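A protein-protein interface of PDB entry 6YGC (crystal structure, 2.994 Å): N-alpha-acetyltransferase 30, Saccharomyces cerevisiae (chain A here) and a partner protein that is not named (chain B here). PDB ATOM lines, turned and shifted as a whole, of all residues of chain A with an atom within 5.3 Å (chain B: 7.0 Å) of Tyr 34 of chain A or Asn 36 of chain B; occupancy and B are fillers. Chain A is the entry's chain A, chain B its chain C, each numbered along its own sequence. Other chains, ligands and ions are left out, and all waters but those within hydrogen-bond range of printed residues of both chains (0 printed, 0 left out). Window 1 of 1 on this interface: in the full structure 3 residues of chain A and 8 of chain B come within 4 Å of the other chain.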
ATOM      1  N   SER A  32     -31.674   5.254  21.079  1.00  0.00           N
ATOM      2  CA  SER A  32     -31.242   5.025  22.445  1.00  0.00           C
ATOM      3  C   SER A  32     -31.790   6.124  23.351  1.00  0.00           C
ATOM      4  O   SER A  32     -32.376   7.108  22.893  1.00  0.00           O
ATOM      5  CB  SER A  32     -29.717   4.969  22.526  1.00  0.00           C
ATOM      6  OG  SER A  32     -29.142   6.181  22.070  1.00  0.00           O
ATOM      7  N   ILE A  33     -31.591   5.951  24.660  1.00  0.00           N
ATOM      8  CA  ILE A  33     -32.156   6.905  25.608  1.00  0.00           C
ATOM      9  C   ILE A  33     -31.449   8.253  25.514  1.00  0.00           C
ATOM     10  O   ILE A  33     -32.052   9.298  25.786  1.00  0.00           O
ATOM     11  CB  ILE A  33     -32.112   6.332  27.038  1.00  0.00           C
ATOM     12  CG1 ILE A  33     -32.887   7.234  28.002  1.00  0.00           C
ATOM     13  CG2 ILE A  33     -30.675   6.140  27.505  1.00  0.00           C
ATOM     14  CD1 ILE A  33     -33.014   6.676  29.401  1.00  0.00           C
ATOM     15  N   TYR A  34     -30.175   8.265  25.118  1.00  0.00           N
ATOM     16  CA  TYR A  34     -29.456   9.523  24.967  1.00  0.00           C
ATOM     17  C   TYR A  34     -29.782  10.235  23.662  1.00  0.00           C
ATOM     18  O   TYR A  34     -29.420  11.409  23.510  1.00  0.00           O
ATOM     19  CB  TYR A  34     -27.948   9.289  25.087  1.00  0.00           C
ATOM     20  CG  TYR A  34     -27.461   9.371  26.515  1.00  0.00           C
ATOM     21  CD1 TYR A  34     -27.565   8.281  27.368  1.00  0.00           C
ATOM     22  CD2 TYR A  34     -26.914  10.546  27.016  1.00  0.00           C
ATOM     23  CE1 TYR A  34     -27.130   8.356  28.676  1.00  0.00           C
ATOM     24  CE2 TYR A  34     -26.477  10.629  28.322  1.00  0.00           C
ATOM     25  CZ  TYR A  34     -26.587   9.531  29.147  1.00  0.00           C
ATOM     26  OH  TYR A  34     -26.152   9.610  30.448  1.00  0.00           O
ATOM     27  N   VAL A  35     -30.445   9.561  22.721  1.00  0.00           N
ATOM     28  CA  VAL A  35     -31.029  10.267  21.586  1.00  0.00           C
ATOM     29  C   VAL A  35     -32.158  11.171  22.063  1.00  0.00           C
ATOM     30  O   VAL A  35     -32.292  12.315  21.609  1.00  0.00           O
ATOM     31  CB  VAL A  35     -31.519   9.264  20.526  1.00  0.00           C
ATOM     32  CG1 VAL A  35     -32.280   9.982  19.420  1.00  0.00           C
ATOM     33  CG2 VAL A  35     -30.352   8.483  19.950  1.00  0.00           C
ATOM     34  N   TYR A  36     -32.975  10.679  22.997  1.00  0.00           N
ATOM     35  CA  TYR A  36     -34.067  11.486  23.531  1.00  0.00           C
ATOM     36  C   TYR A  36     -33.543  12.603  24.424  1.00  0.00           C
ATOM     37  O   TYR A  36     -34.047  13.730  24.376  1.00  0.00           O
ATOM     38  CB  TYR A  36     -35.047  10.603  24.302  1.00  0.00           C
ATOM     39  CG  TYR A  36     -35.799   9.615  23.441  1.00  0.00           C
ATOM     40  CD1 TYR A  36     -36.941   9.997  22.749  1.00  0.00           C
ATOM     41  CD2 TYR A  36     -35.372   8.298  23.326  1.00  0.00           C
ATOM     42  CE1 TYR A  36     -37.636   9.097  21.962  1.00  0.00           C
ATOM     43  CE2 TYR A  36     -36.060   7.389  22.542  1.00  0.00           C
ATOM     44  CZ  TYR A  36     -37.191   7.795  21.862  1.00  0.00           C
ATOM     45  OH  TYR A  36     -37.881   6.898  21.080  1.00  0.00           O
ATOM     46  N   ARG A  37     -32.532  12.312  25.247  1.00  0.00           N
ATOM     47  CA  ARG A  37     -31.984  13.333  26.131  1.00  0.00           C
ATOM     48  C   ARG A  37     -31.173  14.379  25.378  1.00  0.00           C
ATOM     49  O   ARG A  37     -30.917  15.455  25.926  1.00  0.00           O
ATOM     50  CB  ARG A  37     -31.129  12.690  27.225  1.00  0.00           C
ATOM     51  CG  ARG A  37     -31.940  11.954  28.284  1.00  0.00           C
ATOM     52  CD  ARG A  37     -31.441  12.276  29.686  1.00  0.00           C
ATOM     53  NE  ARG A  37     -32.250  11.639  30.722  1.00  0.00           N
ATOM     54  CZ  ARG A  37     -33.354  12.168  31.242  1.00  0.00           C
ATOM     55  NH1 ARG A  37     -33.788  13.347  30.821  1.00  0.00           N
ATOM     56  NH2 ARG A  37     -34.025  11.517  32.181  1.00  0.00           N
ATOM     57  N   TYR A  38     -30.759  14.091  24.143  1.00  0.00           N
ATOM     58  CA  TYR A  38     -30.155  15.131  23.317  1.00  0.00           C
ATOM     59  C   TYR A  38     -31.190  16.172  22.908  1.00  0.00           C
ATOM     60  O   TYR A  38     -30.917  17.377  22.944  1.00  0.00           O
ATOM     61  CB  TYR A  38     -29.498  14.509  22.085  1.00  0.00           C
ATOM     62  CG  TYR A  38     -29.298  15.478  20.942  1.00  0.00           C
ATOM     63  CD1 TYR A  38     -28.251  16.389  20.951  1.00  0.00           C
ATOM     64  CD2 TYR A  38     -30.156  15.478  19.849  1.00  0.00           C
ATOM     65  CE1 TYR A  38     -28.068  17.278  19.909  1.00  0.00           C
ATOM     66  CE2 TYR A  38     -29.980  16.362  18.803  1.00  0.00           C
ATOM     67  CZ  TYR A  38     -28.934  17.258  18.836  1.00  0.00           C
ATOM     68  OH  TYR A  38     -28.755  18.139  17.793  1.00  0.00           O
ATOM     69  N   LEU B  28     -16.462   6.939  31.104  1.00  0.00           N
ATOM     70  CA  LEU B  28     -17.746   7.594  31.315  1.00  0.00           C
ATOM     71  C   LEU B  28     -17.784   8.926  30.576  1.00  0.00           C
ATOM     72  O   LEU B  28     -16.891   9.762  30.738  1.00  0.00           O
ATOM     73  CB  LEU B  28     -17.993   7.811  32.807  1.00  0.00           C
ATOM     74  CG  LEU B  28     -19.331   8.450  33.190  1.00  0.00           C
ATOM     75  CD1 LEU B  28     -20.479   7.472  32.988  1.00  0.00           C
ATOM     76  CD2 LEU B  28     -19.303   8.964  34.622  1.00  0.00           C
ATOM     77  N   VAL B  29     -18.825   9.123  29.768  1.00  0.00           N
ATOM     78  CA  VAL B  29     -18.993  10.339  28.988  1.00  0.00           C
ATOM     79  C   VAL B  29     -20.084  11.234  29.566  1.00  0.00           C
ATOM     80  O   VAL B  29     -19.917  12.454  29.634  1.00  0.00           O
ATOM     81  CB  VAL B  29     -19.281  10.007  27.508  1.00  0.00           C
ATOM     82  CG1 VAL B  29     -19.428  11.285  26.698  1.00  0.00           C
ATOM     83  CG2 VAL B  29     -18.180   9.132  26.935  1.00  0.00           C
ATOM     84  N   ALA B  30     -21.206  10.652  29.986  1.00  0.00           N
ATOM     85  CA  ALA B  30     -22.311  11.441  30.510  1.00  0.00           C
ATOM     86  C   ALA B  30     -23.145  10.597  31.461  1.00  0.00           C
ATOM     87  O   ALA B  30     -23.154   9.366  31.389  1.00  0.00           O
ATOM     88  CB  ALA B  30     -23.190  12.000  29.384  1.00  0.00           C
ATOM     89  N   VAL B  31     -23.851  11.286  32.355  1.00  0.00           N
ATOM     90  CA  VAL B  31     -24.772  10.655  33.295  1.00  0.00           C
ATOM     91  C   VAL B  31     -25.857  11.668  33.638  1.00  0.00           C
ATOM     92  O   VAL B  31     -25.585  12.864  33.780  1.00  0.00           O
ATOM     93  CB  VAL B  31     -24.038  10.141  34.555  1.00  0.00           C
ATOM     94  CG1 VAL B  31     -23.358  11.284  35.296  1.00  0.00           C
ATOM     95  CG2 VAL B  31     -24.999   9.393  35.471  1.00  0.00           C
ATOM     96  N   ASP B  32     -27.096  11.192  33.750  1.00  0.00           N
ATOM     97  CA  ASP B  32     -28.247  12.053  33.972  1.00  0.00           C
ATOM     98  C   ASP B  32     -28.790  11.856  35.387  1.00  0.00           C
ATOM     99  O   ASP B  32     -28.204  11.142  36.210  1.00  0.00           O
ATOM    100  CB  ASP B  32     -29.318  11.791  32.907  1.00  0.00           C
ATOM    101  CG  ASP B  32     -29.794  10.350  32.892  1.00  0.00           C
ATOM    102  OD1 ASP B  32     -29.242   9.525  33.651  1.00  0.00           O
ATOM    103  OD2 ASP B  32     -30.722  10.041  32.115  1.00  0.00           O
ATOM    104  N   ALA B  33     -29.928  12.495  35.670  1.00  0.00           N
ATOM    105  CA  ALA B  33     -30.504  12.417  37.008  1.00  0.00           C
ATOM    106  C   ALA B  33     -31.154  11.067  37.267  1.00  0.00           C
ATOM    107  O   ALA B  33     -31.280  10.655  38.426  1.00  0.00           O
ATOM    108  CB  ALA B  33     -31.521  13.535  37.214  1.00  0.00           C
ATOM    109  N   GLN B  34     -31.585  10.374  36.216  1.00  0.00           N
ATOM    110  CA  GLN B  34     -32.133   9.033  36.355  1.00  0.00           C
ATOM    111  C   GLN B  34     -31.046   7.964  36.391  1.00  0.00           C
ATOM    112  O   GLN B  34     -31.366   6.770  36.396  1.00  0.00           O
ATOM    113  CB  GLN B  34     -33.118   8.751  35.216  1.00  0.00           C
ATOM    114  CG  GLN B  34     -34.230   7.777  35.577  1.00  0.00           C
ATOM    115  CD  GLN B  34     -35.250   7.618  34.468  1.00  0.00           C
ATOM    116  OE1 GLN B  34     -35.189   8.303  33.446  1.00  0.00           O
ATOM    117  NE2 GLN B  34     -36.199   6.711  34.666  1.00  0.00           N
ATOM    118  N   MET B  35     -29.779   8.381  36.416  1.00  0.00           N
ATOM    119  CA  MET B  35     -28.625   7.481  36.475  1.00  0.00           C
ATOM    120  C   MET B  35     -28.581   6.549  35.263  1.00  0.00           C
ATOM    121  O   MET B  35     -28.476   5.328  35.388  1.00  0.00           O
ATOM    122  CB  MET B  35     -28.603   6.687  37.785  1.00  0.00           C
ATOM    123  CG  MET B  35     -27.228   6.139  38.145  1.00  0.00           C
ATOM    124  SD  MET B  35     -27.217   5.191  39.677  1.00  0.00           S
ATOM    125  CE  MET B  35     -28.215   3.779  39.212  1.00  0.00           C
ATOM    126  N   ASN B  36     -28.666   7.144  34.076  1.00  0.00           N
ATOM    127  CA  ASN B  36     -28.410   6.441  32.826  1.00  0.00           C
ATOM    128  C   ASN B  36     -27.006   6.797  32.356  1.00  0.00           C
ATOM    129  O   ASN B  36     -26.649   7.978  32.295  1.00  0.00           O
ATOM    130  CB  ASN B  36     -29.445   6.804  31.762  1.00  0.00           C
ATOM    131  CG  ASN B  36     -30.869   6.566  32.226  1.00  0.00           C
ATOM    132  OD1 ASN B  36     -31.302   5.424  32.383  1.00  0.00           O
ATOM    133  ND2 ASN B  36     -31.610   7.648  32.440  1.00  0.00           N
ATOM    134  N   LEU B  37     -26.215   5.780  32.037  1.00  0.00           N
ATOM    135  CA  LEU B  37     -24.797   5.957  31.759  1.00  0.00           C
ATOM    136  C   LEU B  37     -24.530   5.940  30.261  1.00  0.00           C
ATOM    137  O   LEU B  37     -25.140   5.167  29.517  1.00  0.00           O
ATOM    138  CB  LEU B  37     -23.972   4.865  32.441  1.00  0.00           C
ATOM    139  CG  LEU B  37     -24.098   4.752  33.961  1.00  0.00           C
ATOM    140  CD1 LEU B  37     -23.344   3.534  34.461  1.00  0.00           C
ATOM    141  CD2 LEU B  37     -23.592   6.015  34.640  1.00  0.00           C
ATOM    142  N   LEU B  38     -23.612   6.800  29.828  1.00  0.00           N
ATOM    143  CA  LEU B  38     -23.105   6.808  28.461  1.00  0.00           C
ATOM    144  C   LEU B  38     -21.605   6.570  28.520  1.00  0.00           C
ATOM    145  O   LEU B  38     -20.870   7.369  29.111  1.00  0.00           O
ATOM    146  CB  LEU B  38     -23.416   8.130  27.757  1.00  0.00           C
ATOM    147  CG  LEU B  38     -23.034   8.201  26.277  1.00  0.00           C
ATOM    148  CD1 LEU B  38     -23.875   7.232  25.461  1.00  0.00           C
ATOM    149  CD2 LEU B  38     -23.174   9.620  25.742  1.00  0.00           C
ATOM    150  N   LEU B  39     -21.155   5.474  27.917  1.00  0.00           N
ATOM    151  CA  LEU B  39     -19.761   5.067  27.973  1.00  0.00           C
ATOM    152  C   LEU B  39     -19.175   4.996  26.569  1.00  0.00           C
ATOM    153  O   LEU B  39     -19.863   4.641  25.608  1.00  0.00           O
ATOM    154  CB  LEU B  39     -19.611   3.707  28.663  1.00  0.00           C
ATOM    155  CG  LEU B  39     -20.255   3.521  30.037  1.00  0.00           C
ATOM    156  CD1 LEU B  39     -20.180   2.063  30.461  1.00  0.00           C
ATOM    157  CD2 LEU B  39     -19.591   4.414  31.071  1.00  0.00           C
ATOM    158  N   VAL B  56     -21.692   3.051  24.039  1.00  0.00           N
ATOM    159  CA  VAL B  56     -22.837   2.294  24.526  1.00  0.00           C
ATOM    160  C   VAL B  56     -23.534   3.094  25.620  1.00  0.00           C
ATOM    161  O   VAL B  56     -22.894   3.797  26.406  1.00  0.00           O
ATOM    162  CB  VAL B  56     -22.424   0.902  25.054  1.00  0.00           C
ATOM    163  CG1 VAL B  56     -23.648   0.049  25.344  1.00  0.00           C
ATOM    164  CG2 VAL B  56     -21.506   0.201  24.064  1.00  0.00           C
ATOM    165  N   SER B  57     -24.859   2.982  25.663  1.00  0.00           N
ATOM    166  CA  SER B  57     -25.674   3.591  26.702  1.00  0.00           C
ATOM    167  C   SER B  57     -26.213   2.512  27.626  1.00  0.00           C
ATOM    168  O   SER B  57     -26.705   1.478  27.165  1.00  0.00           O
ATOM    169  CB  SER B  57     -26.839   4.385  26.102  1.00  0.00           C
ATOM    170  OG  SER B  57     -27.666   4.904  27.127  1.00  0.00           O
ATOM    171  N   VAL B  58     -26.122   2.756  28.930  1.00  0.00           N
ATOM    172  CA  VAL B  58     -26.556   1.771  29.921  1.00  0.00           C
ATOM    173  C   VAL B  58     -27.686   2.357  30.760  1.00  0.00           C
ATOM    174  O   VAL B  58     -27.466   3.331  31.493  1.00  0.00           O
ATOM    175  CB  VAL B  58     -25.382   1.325  30.806  1.00  0.00           C
ATOM    176  CG1 VAL B  58     -25.702   0.006  31.481  1.00  0.00           C
ATOM    177  CG2 VAL B  58     -24.101   1.217  29.998  1.00  0.00           C
ATOM    178  N   PRO B  59     -28.899   1.818  30.677  1.00  0.00           N
ATOM    179  CA  PRO B  59     -29.982   2.290  31.546  1.00  0.00           C
ATOM    180  C   PRO B  59     -29.746   1.882  32.993  1.00  0.00           C
ATOM    181  O   PRO B  59     -28.913   1.031  33.310  1.00  0.00           O
ATOM    182  CB  PRO B  59     -31.227   1.606  30.970  1.00  0.00           C
ATOM    183  CG  PRO B  59     -30.847   1.219  29.573  1.00  0.00           C
ATOM    184  CD  PRO B  59     -29.391   0.890  29.644  1.00  0.00           C
ATOM    185  N   ARG B  60     -30.520   2.506  33.883  1.00  0.00           N
ATOM    186  CA  ARG B  60     -30.358   2.262  35.314  1.00  0.00           C
ATOM    187  C   ARG B  60     -30.719   0.827  35.684  1.00  0.00           C
ATOM    188  O   ARG B  60     -30.004   0.185  36.463  1.00  0.00           O
ATOM    189  CB  ARG B  60     -31.211   3.251  36.113  1.00  0.00           C
ATOM    190  CG  ARG B  60     -31.363   2.898  37.588  1.00  0.00           C
ATOM    191  CD  ARG B  60     -32.313   3.856  38.293  1.00  0.00           C
ATOM    192  NE  ARG B  60     -32.678   3.385  39.628  1.00  0.00           N
ATOM    193  CZ  ARG B  60     -32.094   3.788  40.752  1.00  0.00           C
ATOM    194  NH1 ARG B  60     -31.111   4.677  40.712  1.00  0.00           N
ATOM    195  NH2 ARG B  60     -32.496   3.305  41.920  1.00  0.00           N
ATOM    196  N   ARG B  61     -31.819   0.307  35.133  1.00  0.00           N
ATOM    197  CA  ARG B  61     -32.257  -1.040  35.486  1.00  0.00           C
ATOM    198  C   ARG B  61     -31.245  -2.094  35.055  1.00  0.00           C
ATOM    199  O   ARG B  61     -31.074  -3.109  35.740  1.00  0.00           O
ATOM    200  CB  ARG B  61     -33.619  -1.334  34.855  1.00  0.00           C
ATOM    201  CG  ARG B  61     -34.269  -2.609  35.364  1.00  0.00           C
ATOM    202  CD  ARG B  61     -35.098  -3.291  34.285  1.00  0.00           C
ATOM    203  NE  ARG B  61     -34.262  -3.788  33.196  1.00  0.00           N
ATOM    204  CZ  ARG B  61     -34.696  -4.588  32.227  1.00  0.00           C
ATOM    205  NH1 ARG B  61     -35.959  -4.991  32.212  1.00  0.00           N
ATOM    206  NH2 ARG B  61     -33.863  -4.990  31.276  1.00  0.00           N
ATOM    207  N   VAL B  63     -28.052  -1.928  35.065  1.00  0.00           N
ATOM    208  CA  VAL B  63     -26.830  -1.908  35.862  1.00  0.00           C
ATOM    209  C   VAL B  63     -27.004  -2.790  37.090  1.00  0.00           C
ATOM    210  O   VAL B  63     -28.048  -2.762  37.753  1.00  0.00           O
ATOM    211  CB  VAL B  63     -26.468  -0.466  36.262  1.00  0.00           C
ATOM    212  CG1 VAL B  63     -25.232  -0.449  37.150  1.00  0.00           C
ATOM    213  CG2 VAL B  63     -26.248   0.388  35.030  1.00  0.00           C
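The side-chain carboxylate (OD2) of Asp 32 of chain B is in salt-bridge range of the guanidinium group (NE) of Arg 37 of chain A. The side-chain hydroxyl of Tyr 34 of chain A lies within hydrogen-bond range of the backbone carbonyl oxygen of Ala 30 of chain B, at 3.2 Å. OH of Tyr 34 of chain A sits close to N of Val 31 of chain B (3.4 Å). The backbone carbonyl oxygen of Asn 36 of chain B sits at hydrogen-bond distance from the side-chain hydroxyl of Tyr 34 of chain A (2.5 Å).
The backbone NH (N) of Val 29 of chain B is in hydrogen-bond range of the backbone carbonyl oxygen (O) of Leu 38 of chain B (2.8 Å). OD1 of Asn 36 of chain B is in hydrogen-bond range of N of Arg 60 of chain B (3.4 Å). The backbone carbonyl oxygen (O) of Ala 30 of chain B sits at hydrogen-bond distance from the backbone NH (N) of Leu 38 of chain B, at 3.0 Å. OD1 of Asp 32 of chain B lies within hydrogen-bond range of N of Asn 36 of chain B (2.5 Å). OG of Ser 57 of chain B lies close to O of Leu 37 of chain B, 3.5 Å away. The side-chain carboxylate of Asp 32 of chain B lies within hydrogen-bond range of the backbone NH of Met 35 of chain B (3.0 Å).
Hydrophobic or aromatic side chains of chain A that line the printed part of chain B: Ile 33 and Tyr 34. Of the 19 printed residues of chain B, 8 touch a printed residue of chain A. Among the printed residues, 11 pairs touch across the chains.
Among the printed residues, pairs that only touch across the chains: Ile 33 of chain A with Ser 57 of chain B (3.3 Å), Tyr 34 of chain A with Ser 57 of chain B (3.4 Å), Ile 33 of chain A with Asn 36 of chain B (3.5 Å), Arg 37 of chain A with Gln 34 of chain B (3.6 Å), Tyr 34 of chain A with Leu 38 of chain B (3.7 Å), Tyr 34 of chain A with Asp 32 of chain B (3.8 Å) and Tyr 34 of chain A with Leu 37 of chain B (3.9 Å).
Printed residues of chain B within 4 Å of Tyr 34 of chain A: Ala 30, Val 31, Asp 32, Asn 36, Leu 37, Leu 38 and Ser 57. Of the printed residues of chain A, Asn 36 of chain B touches Ile 33 and Tyr 34. Of the printed residues of chain A, Leu 38 of chain B touches Tyr 34 (3.7 Å). Of the printed residues of chain B, Ile 33 of chain A touches Asn 36 and Ser 57. Ser 32 of chain A touches none of the printed residues of chain B. The nearest residue of chain A that does not touch Asn 36 of chain B is Arg 37 of chain A (4.4 Å).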
